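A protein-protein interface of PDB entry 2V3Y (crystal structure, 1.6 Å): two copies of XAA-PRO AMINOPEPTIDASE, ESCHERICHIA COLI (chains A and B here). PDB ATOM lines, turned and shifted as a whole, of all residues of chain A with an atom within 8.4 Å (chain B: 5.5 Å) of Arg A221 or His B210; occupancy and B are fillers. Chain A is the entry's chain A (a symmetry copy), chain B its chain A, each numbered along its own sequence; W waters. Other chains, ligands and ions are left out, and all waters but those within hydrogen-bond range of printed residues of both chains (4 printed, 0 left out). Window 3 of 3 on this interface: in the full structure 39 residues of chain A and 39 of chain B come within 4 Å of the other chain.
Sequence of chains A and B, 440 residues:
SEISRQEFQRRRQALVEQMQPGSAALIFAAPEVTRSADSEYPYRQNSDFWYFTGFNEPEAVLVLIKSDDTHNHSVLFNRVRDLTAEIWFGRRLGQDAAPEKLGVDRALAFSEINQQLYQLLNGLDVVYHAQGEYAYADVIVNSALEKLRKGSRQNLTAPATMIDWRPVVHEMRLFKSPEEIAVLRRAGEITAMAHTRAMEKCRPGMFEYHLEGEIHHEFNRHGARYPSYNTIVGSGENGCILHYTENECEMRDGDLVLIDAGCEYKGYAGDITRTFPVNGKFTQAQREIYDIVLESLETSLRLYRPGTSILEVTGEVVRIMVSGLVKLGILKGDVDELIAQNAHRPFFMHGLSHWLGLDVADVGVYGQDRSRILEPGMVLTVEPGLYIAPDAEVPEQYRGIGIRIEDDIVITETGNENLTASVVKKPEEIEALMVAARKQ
The backbone carbonyl oxygen (O) of Tyr B209 lies within hydrogen-bond range of the side-chain amide nitrogen (ND2) of Asn A220 (2.9 Å).
O of Arg A221 lies within hydrogen-bond range of NE2 of His B210, at 2.9 Å.
NH2 of Arg A225 lies within salt-bridge range of OE1 of Glu B212 (2.8 Å).
The side-chain carboxylate (OE2) of Glu B214 sits at hydrogen-bond distance from a ring nitrogen (NE2) of His A217 (2.8 Å).
The backbone NH of Phe B207 is in hydrogen-bond range of a ring nitrogen (ND1) of His B210 (3.1 Å).
ND1 of His A217 lies within hydrogen-bond range of NH1 of Arg A197.
NE of Arg A221 lies within salt-bridge range of OE1 of Glu A218, 2.9 Å away.
Among the printed residues, merely in contact across the chains: His A217 with Gly B213 (3.5 Å), Asn A220 with His B210 (3.7 Å), Asn A220 with Gly B213 (3.6 Å) and Gly A223 with Tyr B209 (3.6 Å).
Ala A194 touches none of the printed residues of chain B.
Printed residues of chain B within 4 Å of Asn A220: Tyr B209, His B210 and Gly B213.
Of the printed residues of chain B, Arg A221 touches His B210 (2.9 Å).
Printed residues of chain B within 4 Å of Gly A223: Tyr B209.
Of the printed residues of chain A, Tyr B209 touches Asn A220 and Gly A223.
Printed residues of chain A within 4 Å of His B210: Asn A220 (3.7 Å) and Arg A221 (2.9 Å).
Printed residues of chain A within 4 Å of Glu B212: Arg A225 (2.8 Å).
The nearest printed residue of chain B that does not touch Arg A221 is Tyr B209 (4.4 Å).
The nearest printed residue of chain A that does not touch His B210 is His A222 (4.9 Å).
The nearest printed residue of chain B that does not touch Asn A220 is Glu B212 (4.4 Å).
Printed residues of chain B that touch a printed residue of chain A: Tyr B209, His B210, Glu B212, Gly B213 and Glu B214.
Hydrophobic or aromatic side chains of chain B that line the printed part of chain A: Tyr B209 and His B210.
Of the 17 printed residues of chain A, 5 touch a printed residue of chain B.
Among the printed residues, 8 pairs touch across the chains.
Positions printed for both chains: 214 and 215.
Water W1 lies within hydrogen-bond range of O of Arg A225 (2.7 Å), ND2 of Asn A220 (2.9 Å) and OE2 of Glu B212 (2.9 Å).
Water W3 lies within hydrogen-bond range of O of Arg A221, OH of Tyr B209 and NE2 of His B210.
Water W2 lies within hydrogen-bond range of the backbone carbonyl oxygen (O) of Gly B213 (2.8 Å) and the backbone NH (N) of His A217 (3.5 Å).
Water W4 lies within hydrogen-bond range of OE2 of Glu B212 and NH2 of Arg A225.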
ATOM      1  N   ARG A 186      -5.183   1.883  15.491  1.00  0.00           N
ATOM      2  CA  ARG A 186      -5.821   2.728  16.487  1.00  0.00           C
ATOM      3  C   ARG A 186      -5.003   4.005  16.697  1.00  0.00           C
ATOM      4  O   ARG A 186      -5.559   5.113  16.812  1.00  0.00           O
ATOM      5  CB  ARG A 186      -6.026   1.981  17.798  1.00  0.00           C
ATOM      6  CG  ARG A 186      -6.774   2.769  18.846  1.00  0.00           C
ATOM      7  CD  ARG A 186      -8.118   3.335  18.363  1.00  0.00           C
ATOM      8  NE  ARG A 186      -8.800   4.102  19.410  1.00  0.00           N
ATOM      9  CZ  ARG A 186      -9.778   4.979  19.187  1.00  0.00           C
ATOM     10  NH1 ARG A 186     -10.198   5.222  17.959  1.00  0.00           N
ATOM     11  NH2 ARG A 186     -10.324   5.641  20.200  1.00  0.00           N
ATOM     12  N   ILE A 190      -6.511   7.754  16.257  1.00  0.00           N
ATOM     13  CA  ILE A 190      -6.395   8.767  17.307  1.00  0.00           C
ATOM     14  C   ILE A 190      -5.658  10.006  16.787  1.00  0.00           C
ATOM     15  O   ILE A 190      -6.075  11.162  16.982  1.00  0.00           O
ATOM     16  CB  ILE A 190      -5.667   8.213  18.535  1.00  0.00           C
ATOM     17  CG1 ILE A 190      -6.517   7.135  19.200  1.00  0.00           C
ATOM     18  CG2 ILE A 190      -5.315   9.357  19.487  1.00  0.00           C
ATOM     19  CD1 ILE A 190      -5.796   6.310  20.267  1.00  0.00           C
ATOM     20  N   MET A 193      -7.855  11.956  14.403  1.00  0.00           N
ATOM     21  CA  MET A 193      -8.891  12.754  15.098  1.00  0.00           C
ATOM     22  C   MET A 193      -8.275  14.056  15.636  1.00  0.00           C
ATOM     23  O   MET A 193      -8.908  15.132  15.611  1.00  0.00           O
ATOM     24  CB  MET A 193      -9.556  11.975  16.235  1.00  0.00           C
ATOM     25  CG  MET A 193     -10.441  10.861  15.754  1.00  0.00           C
ATOM     26  SD  MET A 193     -11.454  10.103  17.049  1.00  0.00           S
ATOM     27  CE  MET A 193     -10.280   8.921  17.680  1.00  0.00           C
ATOM     28  N   ALA A 194      -7.032  13.938  16.120  1.00  0.00           N
ATOM     29  CA  ALA A 194      -6.297  15.107  16.665  1.00  0.00           C
ATOM     30  C   ALA A 194      -6.049  16.159  15.586  1.00  0.00           C
ATOM     31  O   ALA A 194      -6.271  17.353  15.801  1.00  0.00           O
ATOM     32  CB  ALA A 194      -4.982  14.660  17.310  1.00  0.00           C
ATOM     33  N   ARG A 197      -9.284  17.863  14.588  1.00  0.00           N
ATOM     34  CA  ARG A 197      -9.549  18.858  15.636  1.00  0.00           C
ATOM     35  C   ARG A 197      -8.726  20.128  15.439  1.00  0.00           C
ATOM     36  O   ARG A 197      -9.250  21.257  15.564  1.00  0.00           O
ATOM     37  CB  ARG A 197      -9.324  18.245  17.018  1.00  0.00           C
ATOM     38  CG  ARG A 197      -9.567  19.210  18.166  1.00  0.00           C
ATOM     39  CD  ARG A 197      -9.394  18.457  19.468  1.00  0.00           C
ATOM     40  NE  ARG A 197      -9.398  19.360  20.615  1.00  0.00           N
ATOM     41  CZ  ARG A 197      -9.390  18.964  21.888  1.00  0.00           C
ATOM     42  NH1 ARG A 197      -9.476  17.689  22.188  1.00  0.00           N
ATOM     43  NH2 ARG A 197      -9.329  19.872  22.866  1.00  0.00           N
ATOM     44  N   GLU A 214      -4.528  21.508  21.642  1.00  0.00           N
ATOM     45  CA  GLU A 214      -5.703  20.791  21.126  1.00  0.00           C
ATOM     46  C   GLU A 214      -5.356  19.335  20.797  1.00  0.00           C
ATOM     47  O   GLU A 214      -6.074  18.421  21.180  1.00  0.00           O
ATOM     48  CB  GLU A 214      -6.253  21.490  19.876  1.00  0.00           C
ATOM     49  CG  GLU A 214      -6.792  22.895  20.125  1.00  0.00           C
ATOM     50  CD  GLU A 214      -7.951  22.945  21.117  1.00  0.00           C
ATOM     51  OE1 GLU A 214      -8.853  22.114  20.951  1.00  0.00           O
ATOM     52  OE2 GLU A 214      -7.978  23.877  21.988  1.00  0.00           O
ATOM     53  N   ILE A 215      -4.245  19.149  20.088  1.00  0.00           N
ATOM     54  CA  ILE A 215      -3.774  17.835  19.640  1.00  0.00           C
ATOM     55  C   ILE A 215      -3.481  16.917  20.836  1.00  0.00           C
ATOM     56  O   ILE A 215      -3.951  15.784  20.898  1.00  0.00           O
ATOM     57  CB  ILE A 215      -2.570  18.010  18.708  1.00  0.00           C
ATOM     58  CG1 ILE A 215      -3.049  18.598  17.374  1.00  0.00           C
ATOM     59  CG2 ILE A 215      -1.799  16.682  18.520  1.00  0.00           C
ATOM     60  CD1 ILE A 215      -1.927  19.083  16.490  1.00  0.00           C
ATOM     61  N   HIS A 216      -2.691  17.402  21.787  1.00  0.00           N
ATOM     62  CA  HIS A 216      -2.327  16.586  22.952  1.00  0.00           C
ATOM     63  C   HIS A 216      -3.546  16.197  23.807  1.00  0.00           C
ATOM     64  O   HIS A 216      -3.594  15.092  24.367  1.00  0.00           O
ATOM     65  CB  HIS A 216      -1.305  17.336  23.776  1.00  0.00           C
ATOM     66  CG  HIS A 216       0.018  17.488  23.087  1.00  0.00           C
ATOM     67  ND1 HIS A 216       1.066  18.169  23.675  1.00  0.00           N
ATOM     68  CD2 HIS A 216       0.464  17.065  21.880  1.00  0.00           C
ATOM     69  CE1 HIS A 216       2.108  18.141  22.854  1.00  0.00           C
ATOM     70  NE2 HIS A 216       1.774  17.472  21.768  1.00  0.00           N
ATOM     71  N   HIS A 217      -4.510  17.112  23.925  1.00  0.00           N
ATOM     72  CA  HIS A 217      -5.765  16.835  24.656  1.00  0.00           C
ATOM     73  C   HIS A 217      -6.515  15.696  23.947  1.00  0.00           C
ATOM     74  O   HIS A 217      -7.014  14.759  24.586  1.00  0.00           O
ATOM     75  CB  HIS A 217      -6.632  18.091  24.753  1.00  0.00           C
ATOM     76  CG  HIS A 217      -7.882  17.876  25.542  1.00  0.00           C
ATOM     77  ND1 HIS A 217      -9.039  17.365  24.978  1.00  0.00           N
ATOM     78  CD2 HIS A 217      -8.146  18.026  26.864  1.00  0.00           C
ATOM     79  CE1 HIS A 217      -9.970  17.264  25.915  1.00  0.00           C
ATOM     80  NE2 HIS A 217      -9.455  17.663  27.067  1.00  0.00           N
ATOM     81  N   GLU A 218      -6.592  15.788  22.631  1.00  0.00           N
ATOM     82  CA  GLU A 218      -7.248  14.727  21.838  1.00  0.00           C
ATOM     83  C   GLU A 218      -6.546  13.371  22.010  1.00  0.00           C
ATOM     84  O   GLU A 218      -7.198  12.332  22.211  1.00  0.00           O
ATOM     85  CB  GLU A 218      -7.381  15.104  20.384  1.00  0.00           C
ATOM     86  CG  GLU A 218      -8.316  14.143  19.587  1.00  0.00           C
ATOM     87  CD  GLU A 218      -9.800  14.312  19.952  1.00  0.00           C
ATOM     88  OE1 GLU A 218     -10.166  15.324  20.589  1.00  0.00           O
ATOM     89  OE2 GLU A 218     -10.600  13.406  19.599  1.00  0.00           O
ATOM     90  N   PHE A 219      -5.206  13.343  21.919  1.00  0.00           N
ATOM     91  CA  PHE A 219      -4.478  12.111  22.185  1.00  0.00           C
ATOM     92  C   PHE A 219      -4.909  11.522  23.532  1.00  0.00           C
ATOM     93  O   PHE A 219      -5.270  10.349  23.652  1.00  0.00           O
ATOM     94  CB  PHE A 219      -2.991  12.358  22.274  1.00  0.00           C
ATOM     95  CG  PHE A 219      -2.306  12.755  20.982  1.00  0.00           C
ATOM     96  CD1 PHE A 219      -2.929  12.698  19.727  1.00  0.00           C
ATOM     97  CD2 PHE A 219      -0.974  13.178  21.050  1.00  0.00           C
ATOM     98  CE1 PHE A 219      -2.226  13.056  18.562  1.00  0.00           C
ATOM     99  CE2 PHE A 219      -0.273  13.538  19.907  1.00  0.00           C
ATOM    100  CZ  PHE A 219      -0.908  13.483  18.654  1.00  0.00           C
ATOM    101  N   ASN A 220      -4.855  12.378  24.551  1.00  0.00           N
ATOM    102  CA  ASN A 220      -5.133  11.975  25.915  1.00  0.00           C
ATOM    103  C   ASN A 220      -6.513  11.389  26.082  1.00  0.00           C
ATOM    104  O   ASN A 220      -6.671  10.360  26.727  1.00  0.00           O
ATOM    105  CB  ASN A 220      -4.900  13.151  26.880  1.00  0.00           C
ATOM    106  CG  ASN A 220      -5.375  12.860  28.288  1.00  0.00           C
ATOM    107  OD1 ASN A 220      -6.587  12.847  28.547  1.00  0.00           O
ATOM    108  ND2 ASN A 220      -4.435  12.598  29.198  1.00  0.00           N
ATOM    109  N   ARG A 221      -7.529  12.002  25.484  1.00  0.00           N
ATOM    110  CA  ARG A 221      -8.863  11.515  25.796  1.00  0.00           C
ATOM    111  C   ARG A 221      -9.103  10.083  25.289  1.00  0.00           C
ATOM    112  O   ARG A 221      -9.888   9.337  25.880  1.00  0.00           O
ATOM    113  CB  ARG A 221      -9.946  12.493  25.408  1.00  0.00           C
ATOM    114  CG  ARG A 221     -10.104  12.750  23.985  1.00  0.00           C
ATOM    115  CD  ARG A 221     -11.155  13.879  23.793  1.00  0.00           C
ATOM    116  NE  ARG A 221     -11.747  13.791  22.465  1.00  0.00           N
ATOM    117  CZ  ARG A 221     -12.798  13.040  22.143  1.00  0.00           C
ATOM    118  NH1 ARG A 221     -13.452  12.326  23.060  1.00  0.00           N
ATOM    119  NH2 ARG A 221     -13.213  13.023  20.880  1.00  0.00           N
ATOM    120  N   HIS A 222      -8.364   9.702  24.243  1.00  0.00           N
ATOM    121  CA  HIS A 222      -8.456   8.334  23.697  1.00  0.00           C
ATOM    122  C   HIS A 222      -7.465   7.341  24.348  1.00  0.00           C
ATOM    123  O   HIS A 222      -7.369   6.183  23.939  1.00  0.00           O
ATOM    124  CB  HIS A 222      -8.292   8.343  22.182  1.00  0.00           C
ATOM    125  CG  HIS A 222      -9.297   9.195  21.506  1.00  0.00           C
ATOM    126  ND1 HIS A 222     -10.639   8.877  21.507  1.00  0.00           N
ATOM    127  CD2 HIS A 222      -9.186  10.389  20.872  1.00  0.00           C
ATOM    128  CE1 HIS A 222     -11.301   9.819  20.860  1.00  0.00           C
ATOM    129  NE2 HIS A 222     -10.443  10.744  20.458  1.00  0.00           N
ATOM    130  N   GLY A 223      -6.753   7.780  25.379  1.00  0.00           N
ATOM    131  CA  GLY A 223      -5.858   6.920  26.133  1.00  0.00           C
ATOM    132  C   GLY A 223      -4.435   6.856  25.610  1.00  0.00           C
ATOM    133  O   GLY A 223      -3.693   5.928  25.962  1.00  0.00           O
ATOM    134  N   ALA A 224      -4.059   7.787  24.732  1.00  0.00           N
ATOM    135  CA  ALA A 224      -2.668   7.961  24.308  1.00  0.00           C
ATOM    136  C   ALA A 224      -2.156   9.167  25.089  1.00  0.00           C
ATOM    137  O   ALA A 224      -2.321  10.328  24.689  1.00  0.00           O
ATOM    138  CB  ALA A 224      -2.569   8.185  22.825  1.00  0.00           C
ATOM    139  N   ARG A 225      -1.581   8.902  26.259  1.00  0.00           N
ATOM    140  CA  ARG A 225      -1.199   9.980  27.172  1.00  0.00           C
ATOM    141  C   ARG A 225      -0.159  10.947  26.621  1.00  0.00           C
ATOM    142  O   ARG A 225      -0.197  12.150  26.901  1.00  0.00           O
ATOM    143  CB  ARG A 225      -0.630   9.410  28.471  1.00  0.00           C
ATOM    144  CG  ARG A 225      -1.634   9.180  29.563  1.00  0.00           C
ATOM    145  CD  ARG A 225      -0.907   8.569  30.768  1.00  0.00           C
ATOM    146  NE  ARG A 225      -0.574   9.529  31.809  1.00  0.00           N
ATOM    147  CZ  ARG A 225       0.157   9.240  32.890  1.00  0.00           C
ATOM    148  NH1 ARG A 225       0.704   8.026  33.046  1.00  0.00           N
ATOM    149  NH2 ARG A 225       0.359  10.163  33.808  1.00  0.00           N
ATOM    150  N   GLY B 205     -16.487   7.430  36.189  1.00  0.00           N
ATOM    151  CA  GLY B 205     -16.290   6.718  34.925  1.00  0.00           C
ATOM    152  C   GLY B 205     -15.201   7.298  34.037  1.00  0.00           C
ATOM    153  O   GLY B 205     -14.679   6.608  33.162  1.00  0.00           O
ATOM    154  N   MET B 206     -14.887   8.572  34.232  1.00  0.00           N
ATOM    155  CA  MET B 206     -13.720   9.124  33.571  1.00  0.00           C
ATOM    156  C   MET B 206     -12.494   8.462  34.173  1.00  0.00           C
ATOM    157  O   MET B 206     -12.516   7.998  35.317  1.00  0.00           O
ATOM    158  CB  MET B 206     -13.678  10.647  33.756  1.00  0.00           C
ATOM    159  CG  MET B 206     -14.685  11.347  32.851  1.00  0.00           C
ATOM    160  SD  MET B 206     -14.798  13.095  33.220  1.00  0.00           S
ATOM    161  CE  MET B 206     -13.109  13.604  33.024  1.00  0.00           C
ATOM    162  N   PHE B 207     -11.421   8.408  33.397  1.00  0.00           N
ATOM    163  CA  PHE B 207     -10.130   7.917  33.888  1.00  0.00           C
ATOM    164  C   PHE B 207      -9.325   9.035  34.537  1.00  0.00           C
ATOM    165  O   PHE B 207      -9.471  10.211  34.193  1.00  0.00           O
ATOM    166  CB  PHE B 207      -9.334   7.260  32.765  1.00  0.00           C
ATOM    167  CG  PHE B 207      -9.848   5.893  32.410  1.00  0.00           C
ATOM    168  CD1 PHE B 207     -11.015   5.753  31.664  1.00  0.00           C
ATOM    169  CD2 PHE B 207      -9.244   4.759  32.931  1.00  0.00           C
ATOM    170  CE1 PHE B 207     -11.521   4.479  31.374  1.00  0.00           C
ATOM    171  CE2 PHE B 207      -9.733   3.495  32.644  1.00  0.00           C
ATOM    172  CZ  PHE B 207     -10.878   3.359  31.878  1.00  0.00           C
ATOM    173  N   GLU B 208      -8.476   8.658  35.499  1.00  0.00           N
ATOM    174  CA  GLU B 208      -7.602   9.611  36.154  1.00  0.00           C
ATOM    175  C   GLU B 208      -6.864  10.470  35.099  1.00  0.00           C
ATOM    176  O   GLU B 208      -6.760  11.673  35.248  1.00  0.00           O
ATOM    177  CB  GLU B 208      -6.608   8.881  37.073  1.00  0.00           C
ATOM    178  CG  GLU B 208      -7.272   8.277  38.322  1.00  0.00           C
ATOM    179  CD  GLU B 208      -6.428   7.214  39.022  1.00  0.00           C
ATOM    180  OE1 GLU B 208      -5.548   6.613  38.367  1.00  0.00           O
ATOM    181  OE2 GLU B 208      -6.705   6.970  40.221  1.00  0.00           O
ATOM    182  N   TYR B 209      -6.377   9.821  34.035  1.00  0.00           N
ATOM    183  CA  TYR B 209      -5.599  10.541  33.002  1.00  0.00           C
ATOM    184  C   TYR B 209      -6.434  11.590  32.262  1.00  0.00           C
ATOM    185  O   TYR B 209      -5.877  12.555  31.738  1.00  0.00           O
ATOM    186  CB  TYR B 209      -4.909   9.613  32.025  1.00  0.00           C
ATOM    187  CG  TYR B 209      -5.785   8.737  31.200  1.00  0.00           C
ATOM    188  CD1 TYR B 209      -6.437   9.212  30.059  1.00  0.00           C
ATOM    189  CD2 TYR B 209      -5.905   7.391  31.507  1.00  0.00           C
ATOM    190  CE1 TYR B 209      -7.220   8.377  29.267  1.00  0.00           C
ATOM    191  CE2 TYR B 209      -6.689   6.556  30.745  1.00  0.00           C
ATOM    192  CZ  TYR B 209      -7.355   7.039  29.612  1.00  0.00           C
ATOM    193  OH  TYR B 209      -8.131   6.192  28.817  1.00  0.00           O
ATOM    194  N   HIS B 210      -7.764  11.422  32.244  1.00  0.00           N
ATOM    195  CA  HIS B 210      -8.595  12.450  31.612  1.00  0.00           C
ATOM    196  C   HIS B 210      -8.467  13.785  32.316  1.00  0.00           C
ATOM    197  O   HIS B 210      -8.452  14.841  31.657  1.00  0.00           O
ATOM    198  CB  HIS B 210     -10.051  12.054  31.545  1.00  0.00           C
ATOM    199  CG  HIS B 210     -10.329  11.027  30.506  1.00  0.00           C
ATOM    200  ND1 HIS B 210     -11.080   9.900  30.745  1.00  0.00           N
ATOM    201  CD2 HIS B 210      -9.918  10.941  29.219  1.00  0.00           C
ATOM    202  CE1 HIS B 210     -11.150   9.180  29.639  1.00  0.00           C
ATOM    203  NE2 HIS B 210     -10.465   9.795  28.691  1.00  0.00           N
ATOM    204  N   LEU B 211      -8.379  13.774  33.649  1.00  0.00           N
ATOM    205  CA  LEU B 211      -8.207  15.033  34.355  1.00  0.00           C
ATOM    206  C   LEU B 211      -6.823  15.668  34.084  1.00  0.00           C
ATOM    207  O   LEU B 211      -6.680  16.886  34.023  1.00  0.00           O
ATOM    208  CB  LEU B 211      -8.478  14.853  35.850  1.00  0.00           C
ATOM    209  CG  LEU B 211      -9.910  14.384  36.182  1.00  0.00           C
ATOM    210  CD1 LEU B 211     -10.109  14.335  37.719  1.00  0.00           C
ATOM    211  CD2 LEU B 211     -10.983  15.215  35.480  1.00  0.00           C
ATOM    212  N   GLU B 212      -5.803  14.818  34.011  1.00  0.00           N
ATOM    213  CA  GLU B 212      -4.475  15.249  33.541  1.00  0.00           C
ATOM    214  C   GLU B 212      -4.616  15.974  32.182  1.00  0.00           C
ATOM    215  O   GLU B 212      -4.063  17.049  31.975  1.00  0.00           O
ATOM    216  CB  GLU B 212      -3.539  14.047  33.433  1.00  0.00           C
ATOM    217  CG  GLU B 212      -2.238  14.337  32.697  1.00  0.00           C
ATOM    218  CD  GLU B 212      -1.354  13.106  32.609  1.00  0.00           C
ATOM    219  OE1 GLU B 212      -1.352  12.332  33.579  1.00  0.00           O
ATOM    220  OE2 GLU B 212      -0.683  12.887  31.569  1.00  0.00           O
ATOM    221  N   GLY B 213      -5.378  15.382  31.260  1.00  0.00           N
ATOM    222  CA  GLY B 213      -5.556  16.010  29.938  1.00  0.00           C
ATOM    223  C   GLY B 213      -6.195  17.396  30.022  1.00  0.00           C
ATOM    224  O   GLY B 213      -5.751  18.356  29.373  1.00  0.00           O
ATOM    225  N   GLU B 214      -7.249  17.508  30.835  1.00  0.00           N
ATOM    226  CA  GLU B 214      -7.917  18.798  31.056  1.00  0.00           C
ATOM    227  C   GLU B 214      -6.934  19.841  31.597  1.00  0.00           C
ATOM    228  O   GLU B 214      -6.880  20.961  31.108  1.00  0.00           O
ATOM    229  CB  GLU B 214      -9.094  18.636  32.027  1.00  0.00           C
ATOM    230  CG  GLU B 214     -10.221  17.749  31.511  1.00  0.00           C
ATOM    231  CD  GLU B 214     -10.871  18.261  30.228  1.00  0.00           C
ATOM    232  OE1 GLU B 214     -11.163  19.464  30.202  1.00  0.00           O
ATOM    233  OE2 GLU B 214     -11.159  17.427  29.306  1.00  0.00           O
ATOM    234  N   ILE B 215      -6.165  19.443  32.608  1.00  0.00           N
ATOM    235  CA  ILE B 215      -5.198  20.310  33.288  1.00  0.00           C
ATOM    236  C   ILE B 215      -4.118  20.800  32.313  1.00  0.00           C
ATOM    237  O   ILE B 215      -3.840  21.994  32.219  1.00  0.00           O
ATOM    238  CB  ILE B 215      -4.620  19.581  34.506  1.00  0.00           C
ATOM    239  CG1 ILE B 215      -5.702  19.479  35.589  1.00  0.00           C
ATOM    240  CG2 ILE B 215      -3.335  20.270  35.024  1.00  0.00           C
ATOM    241  CD1 ILE B 215      -5.347  18.534  36.711  1.00  0.00           C
HETATM  242  O   HOH W   1      -1.689  13.279  28.825  1.00  0.00           O
HETATM  243  O   HOH W   2      -4.020  17.618  27.311  1.00  0.00           O
HETATM  244  O   HOH W   3     -10.125   6.886  27.031  1.00  0.00           O
HETATM  245  O   HOH W   4       2.014  12.760  32.758  1.00  0.00           O
